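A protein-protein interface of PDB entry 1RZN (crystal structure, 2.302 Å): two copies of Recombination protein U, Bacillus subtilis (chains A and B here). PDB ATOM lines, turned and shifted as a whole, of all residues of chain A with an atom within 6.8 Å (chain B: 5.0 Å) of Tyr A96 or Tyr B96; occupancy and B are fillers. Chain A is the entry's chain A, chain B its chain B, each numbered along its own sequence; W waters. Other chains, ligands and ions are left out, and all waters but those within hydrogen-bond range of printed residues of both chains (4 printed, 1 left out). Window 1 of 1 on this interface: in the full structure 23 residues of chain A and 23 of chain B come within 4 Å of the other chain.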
ATOM      1  N   VAL A  52       3.124  -4.774 -25.560  1.00  0.00           N
ATOM      2  CA  VAL A  52       2.615  -5.260 -26.873  1.00  0.00           C
ATOM      3  C   VAL A  52       2.804  -4.034 -27.752  1.00  0.00           C
ATOM      4  O   VAL A  52       1.938  -3.151 -27.860  1.00  0.00           O
ATOM      5  CB  VAL A  52       1.143  -5.654 -26.830  1.00  0.00           C
ATOM      6  CG1 VAL A  52       0.686  -6.251 -28.125  1.00  0.00           C
ATOM      7  CG2 VAL A  52       0.879  -6.704 -25.720  1.00  0.00           C
ATOM      8  N   HIS A  54       4.502  -2.934 -31.546  1.00  0.00           N
ATOM      9  CA  HIS A  54       4.880  -3.447 -32.889  1.00  0.00           C
ATOM     10  C   HIS A  54       5.412  -2.305 -33.794  1.00  0.00           C
ATOM     11  O   HIS A  54       5.020  -1.162 -33.674  1.00  0.00           O
ATOM     12  CB  HIS A  54       3.673  -4.139 -33.595  1.00  0.00           C
ATOM     13  CG  HIS A  54       3.179  -5.335 -32.870  1.00  0.00           C
ATOM     14  ND1 HIS A  54       3.682  -6.595 -33.113  1.00  0.00           N
ATOM     15  CD2 HIS A  54       2.282  -5.463 -31.847  1.00  0.00           C
ATOM     16  CE1 HIS A  54       3.115  -7.458 -32.270  1.00  0.00           C
ATOM     17  NE2 HIS A  54       2.240  -6.804 -31.517  1.00  0.00           N
ATOM     18  N   LYS A  56       5.126  -0.827 -37.342  1.00  0.00           N
ATOM     19  CA  LYS A  56       4.306  -0.770 -38.519  1.00  0.00           C
ATOM     20  C   LYS A  56       5.169  -1.001 -39.755  1.00  0.00           C
ATOM     21  O   LYS A  56       6.298  -0.465 -39.874  1.00  0.00           O
ATOM     22  CB  LYS A  56       3.620   0.617 -38.679  1.00  0.00           C
ATOM     23  CG  LYS A  56       2.766   1.063 -37.503  1.00  0.00           C
ATOM     24  CD  LYS A  56       2.382   2.535 -37.615  1.00  0.00           C
ATOM     25  CE  LYS A  56       1.307   2.992 -36.609  1.00  0.00           C
ATOM     26  NZ  LYS A  56       0.598   4.259 -37.047  1.00  0.00           N
ATOM     27  N   THR A  85       3.147   8.698 -40.117  1.00  0.00           N
ATOM     28  CA  THR A  85       3.311   8.524 -38.633  1.00  0.00           C
ATOM     29  C   THR A  85       4.707   8.016 -38.240  1.00  0.00           C
ATOM     30  O   THR A  85       5.501   7.664 -39.064  1.00  0.00           O
ATOM     31  CB  THR A  85       2.256   7.561 -38.052  1.00  0.00           C
ATOM     32  OG1 THR A  85       2.553   6.240 -38.489  1.00  0.00           O
ATOM     33  CG2 THR A  85       0.844   7.900 -38.621  1.00  0.00           C
ATOM     34  N   THR A  86       4.944   7.952 -36.946  1.00  0.00           N
ATOM     35  CA  THR A  86       6.026   7.142 -36.375  1.00  0.00           C
ATOM     36  C   THR A  86       5.834   5.670 -36.664  1.00  0.00           C
ATOM     37  O   THR A  86       4.737   5.264 -36.974  1.00  0.00           O
ATOM     38  CB  THR A  86       6.120   7.398 -34.892  1.00  0.00           C
ATOM     39  OG1 THR A  86       4.818   7.298 -34.262  1.00  0.00           O
ATOM     40  CG2 THR A  86       6.588   8.868 -34.615  1.00  0.00           C
ATOM     41  N   TYR A  88       6.551   2.913 -34.553  1.00  0.00           N
ATOM     42  CA  TYR A  88       6.409   2.023 -33.425  1.00  0.00           C
ATOM     43  C   TYR A  88       5.328   2.565 -32.568  1.00  0.00           C
ATOM     44  O   TYR A  88       5.351   3.756 -32.155  1.00  0.00           O
ATOM     45  CB  TYR A  88       7.682   1.920 -32.564  1.00  0.00           C
ATOM     46  CG  TYR A  88       8.867   1.271 -33.298  1.00  0.00           C
ATOM     47  CD1 TYR A  88       9.103  -0.088 -33.249  1.00  0.00           C
ATOM     48  CD2 TYR A  88       9.782   2.034 -33.961  1.00  0.00           C
ATOM     49  CE1 TYR A  88      10.213  -0.653 -33.867  1.00  0.00           C
ATOM     50  CE2 TYR A  88      10.852   1.453 -34.640  1.00  0.00           C
ATOM     51  CZ  TYR A  88      11.112   0.117 -34.510  1.00  0.00           C
ATOM     52  OH  TYR A  88      12.212  -0.455 -35.169  1.00  0.00           O
ATOM     53  N   ASN A  89       4.357   1.703 -32.278  1.00  0.00           N
ATOM     54  CA  ASN A  89       3.417   2.081 -31.224  1.00  0.00           C
ATOM     55  C   ASN A  89       2.870   0.907 -30.513  1.00  0.00           C
ATOM     56  O   ASN A  89       3.097  -0.223 -30.922  1.00  0.00           O
ATOM     57  CB  ASN A  89       2.342   3.023 -31.820  1.00  0.00           C
ATOM     58  CG  ASN A  89       1.229   2.287 -32.636  1.00  0.00           C
ATOM     59  OD1 ASN A  89       1.259   1.046 -32.796  1.00  0.00           O
ATOM     60  ND2 ASN A  89       0.231   3.074 -33.131  1.00  0.00           N
ATOM     61  N   GLY A  90       2.147   1.119 -29.446  1.00  0.00           N
ATOM     62  CA  GLY A  90       1.548  -0.038 -28.798  1.00  0.00           C
ATOM     63  C   GLY A  90       1.099   0.254 -27.401  1.00  0.00           C
ATOM     64  O   GLY A  90       0.935   1.413 -27.087  1.00  0.00           O
ATOM     65  N   ILE A  91       1.018  -0.762 -26.534  1.00  0.00           N
ATOM     66  CA  ILE A  91       0.439  -0.577 -25.190  1.00  0.00           C
ATOM     67  C   ILE A  91       1.284  -1.139 -24.068  1.00  0.00           C
ATOM     68  O   ILE A  91       1.849  -2.190 -24.168  1.00  0.00           O
ATOM     69  CB  ILE A  91      -0.965  -1.254 -25.106  1.00  0.00           C
ATOM     70  CG1 ILE A  91      -1.615  -1.024 -23.750  1.00  0.00           C
ATOM     71  CG2 ILE A  91      -0.903  -2.753 -25.402  1.00  0.00           C
ATOM     72  CD1 ILE A  91      -3.088  -1.421 -23.741  1.00  0.00           C
ATOM     73  N   TYR A  92       1.330  -0.385 -23.009  1.00  0.00           N
ATOM     74  CA  TYR A  92       1.922  -0.735 -21.759  1.00  0.00           C
ATOM     75  C   TYR A  92       1.014  -0.124 -20.639  1.00  0.00           C
ATOM     76  O   TYR A  92       0.849   1.083 -20.547  1.00  0.00           O
ATOM     77  CB  TYR A  92       3.397  -0.237 -21.695  1.00  0.00           C
ATOM     78  CG  TYR A  92       4.122  -0.486 -20.412  1.00  0.00           C
ATOM     79  CD1 TYR A  92       4.485  -1.746 -20.016  1.00  0.00           C
ATOM     80  CD2 TYR A  92       4.432   0.564 -19.595  1.00  0.00           C
ATOM     81  CE1 TYR A  92       5.154  -1.958 -18.825  1.00  0.00           C
ATOM     82  CE2 TYR A  92       5.081   0.386 -18.469  1.00  0.00           C
ATOM     83  CZ  TYR A  92       5.456  -0.873 -18.087  1.00  0.00           C
ATOM     84  OH  TYR A  92       6.084  -0.952 -16.915  1.00  0.00           O
ATOM     85  N   LYS A  93       0.456  -1.002 -19.803  1.00  0.00           N
ATOM     86  CA  LYS A  93      -0.293  -0.590 -18.625  1.00  0.00           C
ATOM     87  C   LYS A  93      -1.400   0.390 -18.934  1.00  0.00           C
ATOM     88  O   LYS A  93      -1.483   1.411 -18.261  1.00  0.00           O
ATOM     89  CB  LYS A  93       0.625   0.049 -17.617  1.00  0.00           C
ATOM     90  CG  LYS A  93       1.546  -0.967 -17.009  1.00  0.00           C
ATOM     91  CD  LYS A  93       2.168  -0.418 -15.778  1.00  0.00           C
ATOM     92  CE  LYS A  93       2.996  -1.446 -15.026  1.00  0.00           C
ATOM     93  NZ  LYS A  93       3.814  -0.754 -14.043  1.00  0.00           N
ATOM     94  N   GLY A  94      -2.219   0.099 -19.947  1.00  0.00           N
ATOM     95  CA  GLY A  94      -3.318   0.985 -20.311  1.00  0.00           C
ATOM     96  C   GLY A  94      -2.938   2.057 -21.344  1.00  0.00           C
ATOM     97  O   GLY A  94      -3.808   2.525 -22.114  1.00  0.00           O
ATOM     98  N   ARG A  95      -1.663   2.428 -21.402  1.00  0.00           N
ATOM     99  CA  ARG A  95      -1.236   3.650 -22.095  1.00  0.00           C
ATOM    100  C   ARG A  95      -0.734   3.361 -23.463  1.00  0.00           C
ATOM    101  O   ARG A  95      -0.302   2.260 -23.787  1.00  0.00           O
ATOM    102  CB  ARG A  95      -0.258   4.468 -21.310  1.00  0.00           C
ATOM    103  CG  ARG A  95      -0.671   4.665 -19.816  1.00  0.00           C
ATOM    104  CD  ARG A  95      -1.052   6.021 -19.291  1.00  0.00           C
ATOM    105  NE  ARG A  95      -0.590   7.211 -20.016  1.00  0.00           N
ATOM    106  CZ  ARG A  95       0.254   8.140 -19.516  1.00  0.00           C
ATOM    107  NH1 ARG A  95       0.799   8.019 -18.304  1.00  0.00           N
ATOM    108  NH2 ARG A  95       0.567   9.203 -20.244  1.00  0.00           N
ATOM    109  N   TYR A  96      -0.972   4.348 -24.310  1.00  0.00           N
ATOM    110  CA  TYR A  96      -0.542   4.340 -25.682  1.00  0.00           C
ATOM    111  C   TYR A  96       0.924   4.801 -25.677  1.00  0.00           C
ATOM    112  O   TYR A  96       1.248   5.876 -25.148  1.00  0.00           O
ATOM    113  CB  TYR A  96      -1.443   5.310 -26.513  1.00  0.00           C
ATOM    114  CG  TYR A  96      -1.003   5.472 -27.981  1.00  0.00           C
ATOM    115  CD1 TYR A  96      -1.261   4.509 -28.906  1.00  0.00           C
ATOM    116  CD2 TYR A  96      -0.277   6.563 -28.391  1.00  0.00           C
ATOM    117  CE1 TYR A  96      -0.861   4.638 -30.181  1.00  0.00           C
ATOM    118  CE2 TYR A  96       0.117   6.714 -29.745  1.00  0.00           C
ATOM    119  CZ  TYR A  96      -0.149   5.735 -30.586  1.00  0.00           C
ATOM    120  OH  TYR A  96       0.265   5.759 -31.860  1.00  0.00           O
ATOM    121  N   ILE A  97       1.767   4.017 -26.322  1.00  0.00           N
ATOM    122  CA  ILE A  97       3.217   4.290 -26.445  1.00  0.00           C
ATOM    123  C   ILE A  97       3.497   4.402 -27.934  1.00  0.00           C
ATOM    124  O   ILE A  97       3.162   3.521 -28.688  1.00  0.00           O
ATOM    125  CB  ILE A  97       4.064   3.083 -25.905  1.00  0.00           C
ATOM    126  CG1 ILE A  97       3.512   2.525 -24.581  1.00  0.00           C
ATOM    127  CG2 ILE A  97       5.625   3.364 -25.851  1.00  0.00           C
ATOM    128  CD1 ILE A  97       3.616   3.427 -23.357  1.00  0.00           C
ATOM    129  N   ASP A  98       4.251   5.403 -28.325  1.00  0.00           N
ATOM    130  CA  ASP A  98       4.486   5.747 -29.696  1.00  0.00           C
ATOM    131  C   ASP A  98       5.882   6.238 -29.797  1.00  0.00           C
ATOM    132  O   ASP A  98       6.253   7.203 -29.158  1.00  0.00           O
ATOM    133  CB  ASP A  98       3.498   6.851 -30.076  1.00  0.00           C
ATOM    134  CG  ASP A  98       3.481   7.159 -31.481  1.00  0.00           C
ATOM    135  OD1 ASP A  98       4.516   7.620 -32.012  1.00  0.00           O
ATOM    136  OD2 ASP A  98       2.476   6.938 -32.180  1.00  0.00           O
ATOM    137  N   PHE A  99       6.682   5.651 -30.684  1.00  0.00           N
ATOM    138  CA  PHE A  99       8.009   6.237 -30.907  1.00  0.00           C
ATOM    139  C   PHE A  99       8.588   5.977 -32.273  1.00  0.00           C
ATOM    140  O   PHE A  99       8.092   5.197 -33.020  1.00  0.00           O
ATOM    141  CB  PHE A  99       9.014   5.788 -29.819  1.00  0.00           C
ATOM    142  CG  PHE A  99       9.214   4.340 -29.768  1.00  0.00           C
ATOM    143  CD1 PHE A  99       8.343   3.529 -29.050  1.00  0.00           C
ATOM    144  CD2 PHE A  99      10.293   3.767 -30.444  1.00  0.00           C
ATOM    145  CE1 PHE A  99       8.547   2.143 -28.984  1.00  0.00           C
ATOM    146  CE2 PHE A  99      10.479   2.402 -30.446  1.00  0.00           C
ATOM    147  CZ  PHE A  99       9.587   1.573 -29.704  1.00  0.00           C
ATOM    148  N   HIS A 122       2.754  14.147 -36.273  1.00  0.00           N
ATOM    149  CA  HIS A 122       2.058  13.008 -35.617  1.00  0.00           C
ATOM    150  C   HIS A 122       2.394  12.991 -34.139  1.00  0.00           C
ATOM    151  O   HIS A 122       1.495  12.862 -33.295  1.00  0.00           O
ATOM    152  CB  HIS A 122       2.429  11.659 -36.291  1.00  0.00           C
ATOM    153  CG  HIS A 122       2.004  10.453 -35.502  1.00  0.00           C
ATOM    154  ND1 HIS A 122       0.688  10.158 -35.241  1.00  0.00           N
ATOM    155  CD2 HIS A 122       2.737   9.490 -34.878  1.00  0.00           C
ATOM    156  CE1 HIS A 122       0.630   9.069 -34.488  1.00  0.00           C
ATOM    157  NE2 HIS A 122       1.859   8.657 -34.237  1.00  0.00           N
ATOM    158  N   VAL A 126       0.009  13.146 -30.922  1.00  0.00           N
ATOM    159  CA  VAL A 126      -0.028  12.171 -29.868  1.00  0.00           C
ATOM    160  C   VAL A 126       0.085  12.794 -28.495  1.00  0.00           C
ATOM    161  O   VAL A 126      -0.611  12.364 -27.539  1.00  0.00           O
ATOM    162  CB  VAL A 126       1.015  11.030 -30.065  1.00  0.00           C
ATOM    163  CG1 VAL A 126       1.111  10.186 -28.847  1.00  0.00           C
ATOM    164  CG2 VAL A 126       0.579  10.172 -31.208  1.00  0.00           C
ATOM    165  N   ASP A 130      -2.112  13.160 -24.655  1.00  0.00           N
ATOM    166  CA  ASP A 130      -1.465  12.615 -23.453  1.00  0.00           C
ATOM    167  C   ASP A 130      -0.864  11.187 -23.608  1.00  0.00           C
ATOM    168  O   ASP A 130      -0.852  10.360 -22.705  1.00  0.00           O
ATOM    169  CB  ASP A 130      -2.374  12.703 -22.214  1.00  0.00           C
ATOM    170  CG  ASP A 130      -1.571  12.713 -20.872  1.00  0.00           C
ATOM    171  OD1 ASP A 130      -0.420  13.245 -20.850  1.00  0.00           O
ATOM    172  OD2 ASP A 130      -2.032  12.211 -19.805  1.00  0.00           O
ATOM    173  N   GLY A 131      -0.248  10.992 -24.738  1.00  0.00           N
ATOM    174  CA  GLY A 131       0.395   9.736 -25.039  1.00  0.00           C
ATOM    175  C   GLY A 131       1.810   9.706 -24.537  1.00  0.00           C
ATOM    176  O   GLY A 131       2.394  10.776 -24.303  1.00  0.00           O
ATOM    177  N   ILE A 132       2.400   8.504 -24.439  1.00  0.00           N
ATOM    178  CA  ILE A 132       3.817   8.448 -24.084  1.00  0.00           C
ATOM    179  C   ILE A 132       4.559   8.422 -25.381  1.00  0.00           C
ATOM    180  O   ILE A 132       4.510   7.432 -26.100  1.00  0.00           O
ATOM    181  CB  ILE A 132       4.086   7.230 -23.230  1.00  0.00           C
ATOM    182  CG1 ILE A 132       3.327   7.411 -21.933  1.00  0.00           C
ATOM    183  CG2 ILE A 132       5.574   7.083 -22.860  1.00  0.00           C
ATOM    184  CD1 ILE A 132       3.401   6.267 -21.037  1.00  0.00           C
ATOM    185  N   CYS A 133       5.286   9.476 -25.688  1.00  0.00           N
ATOM    186  CA  CYS A 133       5.829   9.591 -27.035  1.00  0.00           C
ATOM    187  C   CYS A 133       7.265  10.160 -27.037  1.00  0.00           C
ATOM    188  O   CYS A 133       7.568  11.094 -26.343  1.00  0.00           O
ATOM    189  CB  CYS A 133       4.836  10.463 -27.844  1.00  0.00           C
ATOM    190  SG  CYS A 133       5.223  10.695 -29.538  1.00  0.00           S
ATOM    191  N   ASN B  89      -5.221   1.094 -34.668  1.00  0.00           N
ATOM    192  CA  ASN B  89      -4.916   1.399 -33.283  1.00  0.00           C
ATOM    193  C   ASN B  89      -4.571   2.822 -33.134  1.00  0.00           C
ATOM    194  O   ASN B  89      -4.449   3.527 -34.119  1.00  0.00           O
ATOM    195  CB  ASN B  89      -3.838   0.451 -32.692  1.00  0.00           C
ATOM    196  CG  ASN B  89      -2.365   0.783 -33.132  1.00  0.00           C
ATOM    197  OD1 ASN B  89      -2.079   1.764 -33.815  1.00  0.00           O
ATOM    198  ND2 ASN B  89      -1.419   0.000 -32.585  1.00  0.00           N
ATOM    199  N   GLY B  90      -4.523   3.307 -31.904  1.00  0.00           N
ATOM    200  CA  GLY B  90      -4.174   4.707 -31.763  1.00  0.00           C
ATOM    201  C   GLY B  90      -4.509   5.116 -30.380  1.00  0.00           C
ATOM    202  O   GLY B  90      -4.653   4.242 -29.524  1.00  0.00           O
ATOM    203  N   ILE B  91      -4.747   6.417 -30.204  1.00  0.00           N
ATOM    204  CA  ILE B  91      -4.926   6.983 -28.913  1.00  0.00           C
ATOM    205  C   ILE B  91      -6.096   7.937 -28.837  1.00  0.00           C
ATOM    206  O   ILE B  91      -6.346   8.726 -29.738  1.00  0.00           O
ATOM    207  CB  ILE B  91      -3.633   7.716 -28.460  1.00  0.00           C
ATOM    208  CG1 ILE B  91      -3.803   8.284 -27.036  1.00  0.00           C
ATOM    209  CG2 ILE B  91      -3.309   8.849 -29.384  1.00  0.00           C
ATOM    210  CD1 ILE B  91      -2.618   8.898 -26.427  1.00  0.00           C
ATOM    211  N   GLY B  94      -5.463   9.581 -23.575  1.00  0.00           N
ATOM    212  CA  GLY B  94      -4.484   8.842 -22.789  1.00  0.00           C
ATOM    213  C   GLY B  94      -4.471   7.341 -23.008  1.00  0.00           C
ATOM    214  O   GLY B  94      -3.439   6.726 -22.764  1.00  0.00           O
ATOM    215  N   ARG B  95      -5.568   6.755 -23.499  1.00  0.00           N
ATOM    216  CA  ARG B  95      -5.717   5.298 -23.620  1.00  0.00           C
ATOM    217  C   ARG B  95      -5.396   4.814 -24.945  1.00  0.00           C
ATOM    218  O   ARG B  95      -5.544   5.539 -25.915  1.00  0.00           O
ATOM    219  CB  ARG B  95      -7.121   4.873 -23.323  1.00  0.00           C
ATOM    220  CG  ARG B  95      -7.459   5.381 -21.878  1.00  0.00           C
ATOM    221  CD  ARG B  95      -7.178   4.410 -20.770  1.00  0.00           C
ATOM    222  NE  ARG B  95      -8.469   3.938 -20.193  1.00  0.00           N
ATOM    223  CZ  ARG B  95      -8.984   2.667 -20.241  1.00  0.00           C
ATOM    224  NH1 ARG B  95      -8.371   1.630 -20.830  1.00  0.00           N
ATOM    225  NH2 ARG B  95     -10.174   2.448 -19.692  1.00  0.00           N
ATOM    226  N   TYR B  96      -4.882   3.591 -24.989  1.00  0.00           N
ATOM    227  CA  TYR B  96      -4.607   2.883 -26.212  1.00  0.00           C
ATOM    228  C   TYR B  96      -5.925   2.306 -26.788  1.00  0.00           C
ATOM    229  O   TYR B  96      -6.636   1.615 -26.076  1.00  0.00           O
ATOM    230  CB  TYR B  96      -3.635   1.737 -25.893  1.00  0.00           C
ATOM    231  CG  TYR B  96      -3.313   0.804 -27.087  1.00  0.00           C
ATOM    232  CD1 TYR B  96      -2.265   1.092 -27.970  1.00  0.00           C
ATOM    233  CD2 TYR B  96      -4.022  -0.388 -27.292  1.00  0.00           C
ATOM    234  CE1 TYR B  96      -1.996   0.289 -29.048  1.00  0.00           C
ATOM    235  CE2 TYR B  96      -3.702  -1.245 -28.368  1.00  0.00           C
ATOM    236  CZ  TYR B  96      -2.724  -0.872 -29.250  1.00  0.00           C
ATOM    237  OH  TYR B  96      -2.418  -1.664 -30.298  1.00  0.00           O
ATOM    238  N   ILE B  97      -6.155   2.475 -28.095  1.00  0.00           N
ATOM    239  CA  ILE B  97      -7.385   2.001 -28.772  1.00  0.00           C
ATOM    240  C   ILE B  97      -6.926   1.069 -29.847  1.00  0.00           C
ATOM    241  O   ILE B  97      -5.962   1.332 -30.506  1.00  0.00           O
ATOM    242  CB  ILE B  97      -8.188   3.203 -29.436  1.00  0.00           C
ATOM    243  CG1 ILE B  97      -8.509   4.337 -28.477  1.00  0.00           C
ATOM    244  CG2 ILE B  97      -9.459   2.761 -30.067  1.00  0.00           C
ATOM    245  CD1 ILE B  97      -9.090   3.985 -27.228  1.00  0.00           C
ATOM    246  N   ASP B  98      -7.620  -0.037 -30.030  1.00  0.00           N
ATOM    247  CA  ASP B  98      -7.212  -0.994 -30.977  1.00  0.00           C
ATOM    248  C   ASP B  98      -8.495  -1.685 -31.491  1.00  0.00           C
ATOM    249  O   ASP B  98      -9.390  -1.977 -30.703  1.00  0.00           O
ATOM    250  CB  ASP B  98      -6.274  -1.948 -30.275  1.00  0.00           C
ATOM    251  CG  ASP B  98      -5.598  -2.978 -31.225  1.00  0.00           C
ATOM    252  OD1 ASP B  98      -6.306  -3.875 -31.743  1.00  0.00           O
ATOM    253  OD2 ASP B  98      -4.355  -2.985 -31.495  1.00  0.00           O
ATOM    254  N   HIS B 122      -3.980 -11.225 -30.606  1.00  0.00           N
ATOM    255  CA  HIS B 122      -3.527  -9.844 -30.396  1.00  0.00           C
ATOM    256  C   HIS B 122      -4.526  -9.080 -29.530  1.00  0.00           C
ATOM    257  O   HIS B 122      -4.191  -8.371 -28.523  1.00  0.00           O
ATOM    258  CB  HIS B 122      -3.236  -9.153 -31.769  1.00  0.00           C
ATOM    259  CG  HIS B 122      -2.993  -7.679 -31.625  1.00  0.00           C
ATOM    260  ND1 HIS B 122      -1.827  -7.166 -31.105  1.00  0.00           N
ATOM    261  CD2 HIS B 122      -3.821  -6.627 -31.797  1.00  0.00           C
ATOM    262  CE1 HIS B 122      -1.942  -5.854 -30.975  1.00  0.00           C
ATOM    263  NE2 HIS B 122      -3.135  -5.495 -31.421  1.00  0.00           N
ATOM    264  N   VAL B 126      -4.219  -7.270 -25.918  1.00  0.00           N
ATOM    265  CA  VAL B 126      -4.480  -5.833 -25.732  1.00  0.00           C
ATOM    266  C   VAL B 126      -5.366  -5.615 -24.569  1.00  0.00           C
ATOM    267  O   VAL B 126      -5.042  -4.760 -23.735  1.00  0.00           O
ATOM    268  CB  VAL B 126      -5.047  -5.146 -27.023  1.00  0.00           C
ATOM    269  CG1 VAL B 126      -5.546  -3.763 -26.756  1.00  0.00           C
ATOM    270  CG2 VAL B 126      -3.968  -5.107 -28.031  1.00  0.00           C
ATOM    271  N   GLY B 131      -6.142  -2.172 -22.355  1.00  0.00           N
ATOM    272  CA  GLY B 131      -6.514  -1.317 -23.433  1.00  0.00           C
ATOM    273  C   GLY B 131      -8.016  -1.427 -23.803  1.00  0.00           C
ATOM    274  O   GLY B 131      -8.715  -2.310 -23.435  1.00  0.00           O
ATOM    275  N   ILE B 132      -8.453  -0.486 -24.602  1.00  0.00           N
ATOM    276  CA  ILE B 132      -9.726  -0.522 -25.237  1.00  0.00           C
ATOM    277  C   ILE B 132      -9.628  -1.170 -26.553  1.00  0.00           C
ATOM    278  O   ILE B 132      -9.031  -0.607 -27.468  1.00  0.00           O
ATOM    279  CB  ILE B 132     -10.296   0.888 -25.366  1.00  0.00           C
ATOM    280  CG1 ILE B 132     -10.389   1.512 -23.970  1.00  0.00           C
ATOM    281  CG2 ILE B 132     -11.640   0.723 -25.929  1.00  0.00           C
ATOM    282  CD1 ILE B 132     -10.341   3.135 -23.795  1.00  0.00           C
HETATM  283  O   HOH W   1      -0.932   7.152 -23.195  1.00  0.00           O
HETATM  284  O   HOH W   2       0.436  -8.648 -30.271  1.00  0.00           O
HETATM  285  O   HOH W   3       0.046  -2.982 -30.015  1.00  0.00           O
HETATM  286  O   HOH W   4       1.030  -1.990 -32.161  1.00  0.00           O
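Water W1 lies within hydrogen-bond range of O of Gly B94 (2.6 Å), N of Tyr A96 (3.0 Å), NE of Arg A95 (3.2 Å) and O of Asp A130 (3.2 Å). Water W3 bridges OH of Tyr B96 and O of Val A52. Water W2 bridges a ring nitrogen (ND1) of His B122 (2.8 Å) and a ring nitrogen (NE2) of His A54 (2.9 Å). Water W4 bridges the backbone carbonyl oxygen (O) of Asn A89 (3.0 Å) and the side-chain amide nitrogen (ND2) of Asn B89 (3.2 Å).
Among the printed residues, pairs that only touch across the chains: Val A52 with His B122, Gly A90 with Tyr B96, Ile A91 with Tyr B96, Ile A91 with Val B126, Ile A91 with Gly B131, Gly A94 with Arg B95, Arg A95 with Gly B94, Arg A95 with Tyr B96, Tyr A96 with Gly B90, Tyr A96 with Ile B91, Tyr A96 with Gly B94, Tyr A96 with Tyr B96, Asp A130 with Gly B94 and Gly A131 with Ile B91.
The backbone NH (N) of Ile A132 sits at hydrogen-bond distance from the backbone carbonyl oxygen (O) of Tyr A96 (3.0 Å). N of Ile A91 sits at hydrogen-bond distance from O of Val A52 (2.9 Å). OH of Tyr B96 sits at hydrogen-bond distance from OD2 of Asp B98 (2.6 Å). O of Val B126 is in hydrogen-bond range of N of Gly B131 (3.1 Å). O of Gly B90 lies within hydrogen-bond range of N of Ile B97 (2.7 Å). A ring nitrogen (NE2) of His B122 is in hydrogen-bond range of the side-chain carboxylate of Asp B98, at 2.8 Å.
Of the 12 printed residues of chain B, 9 touch a printed residue of chain A. Printed residues of chain B that touch a printed residue of chain A: Asn B89, Gly B90, Ile B91, Gly B94, Arg B95, Tyr B96, His B122, Val B126 and Gly B131. Among the printed residues, 16 pairs touch across the chains. Among the printed residues, no Asp or Glu carboxylate lies within 4 Å of a Lys or Arg side-chain nitrogen of the other chain.
Ile A91 touches Val B126, but with the chains exchanged Val A126 does not touch Ile B91 (4.2 Å). Ile A91 touches Gly B131, and with the chains exchanged Gly A131 touches Ile B91. Gly A94 touches Arg B95, and with the chains exchanged Arg A95 touches Gly B94. Tyr B96 touches its own counterpart, Tyr A96. 12 positions are printed for both chains. Of the 16 pairs that touch across the chains among the printed residues, 12 have their exchanged pair printed and touching as well.
Tyr A88 touches none of the printed residues of chain B. Of the printed residues of chain B, Gly A90 touches Tyr B96 (3.3 Å). Of the printed residues of chain B, Gly A94 touches Arg B95 (3.7 Å) and Tyr B96 (3.2 Å). Tyr A96 touches four residues of chain B. Asp A98 touches none of the printed residues of chain B. Of the printed residues of chain A, Gly B94 touches Arg A95 (3.8 Å), Tyr A96 (3.8 Å) and Asp A130 (3.9 Å). Printed residues of chain A within 4 Å of Val B126: Ile A91 (3.9 Å).
ND2 of Asn A89 sits at hydrogen-bond distance from OD1 of Asn B89, at 2.7 Å. The backbone carbonyl oxygen (O) of Gly A94 is in hydrogen-bond range of the backbone NH (N) of Tyr B96, 3.2 Å away.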
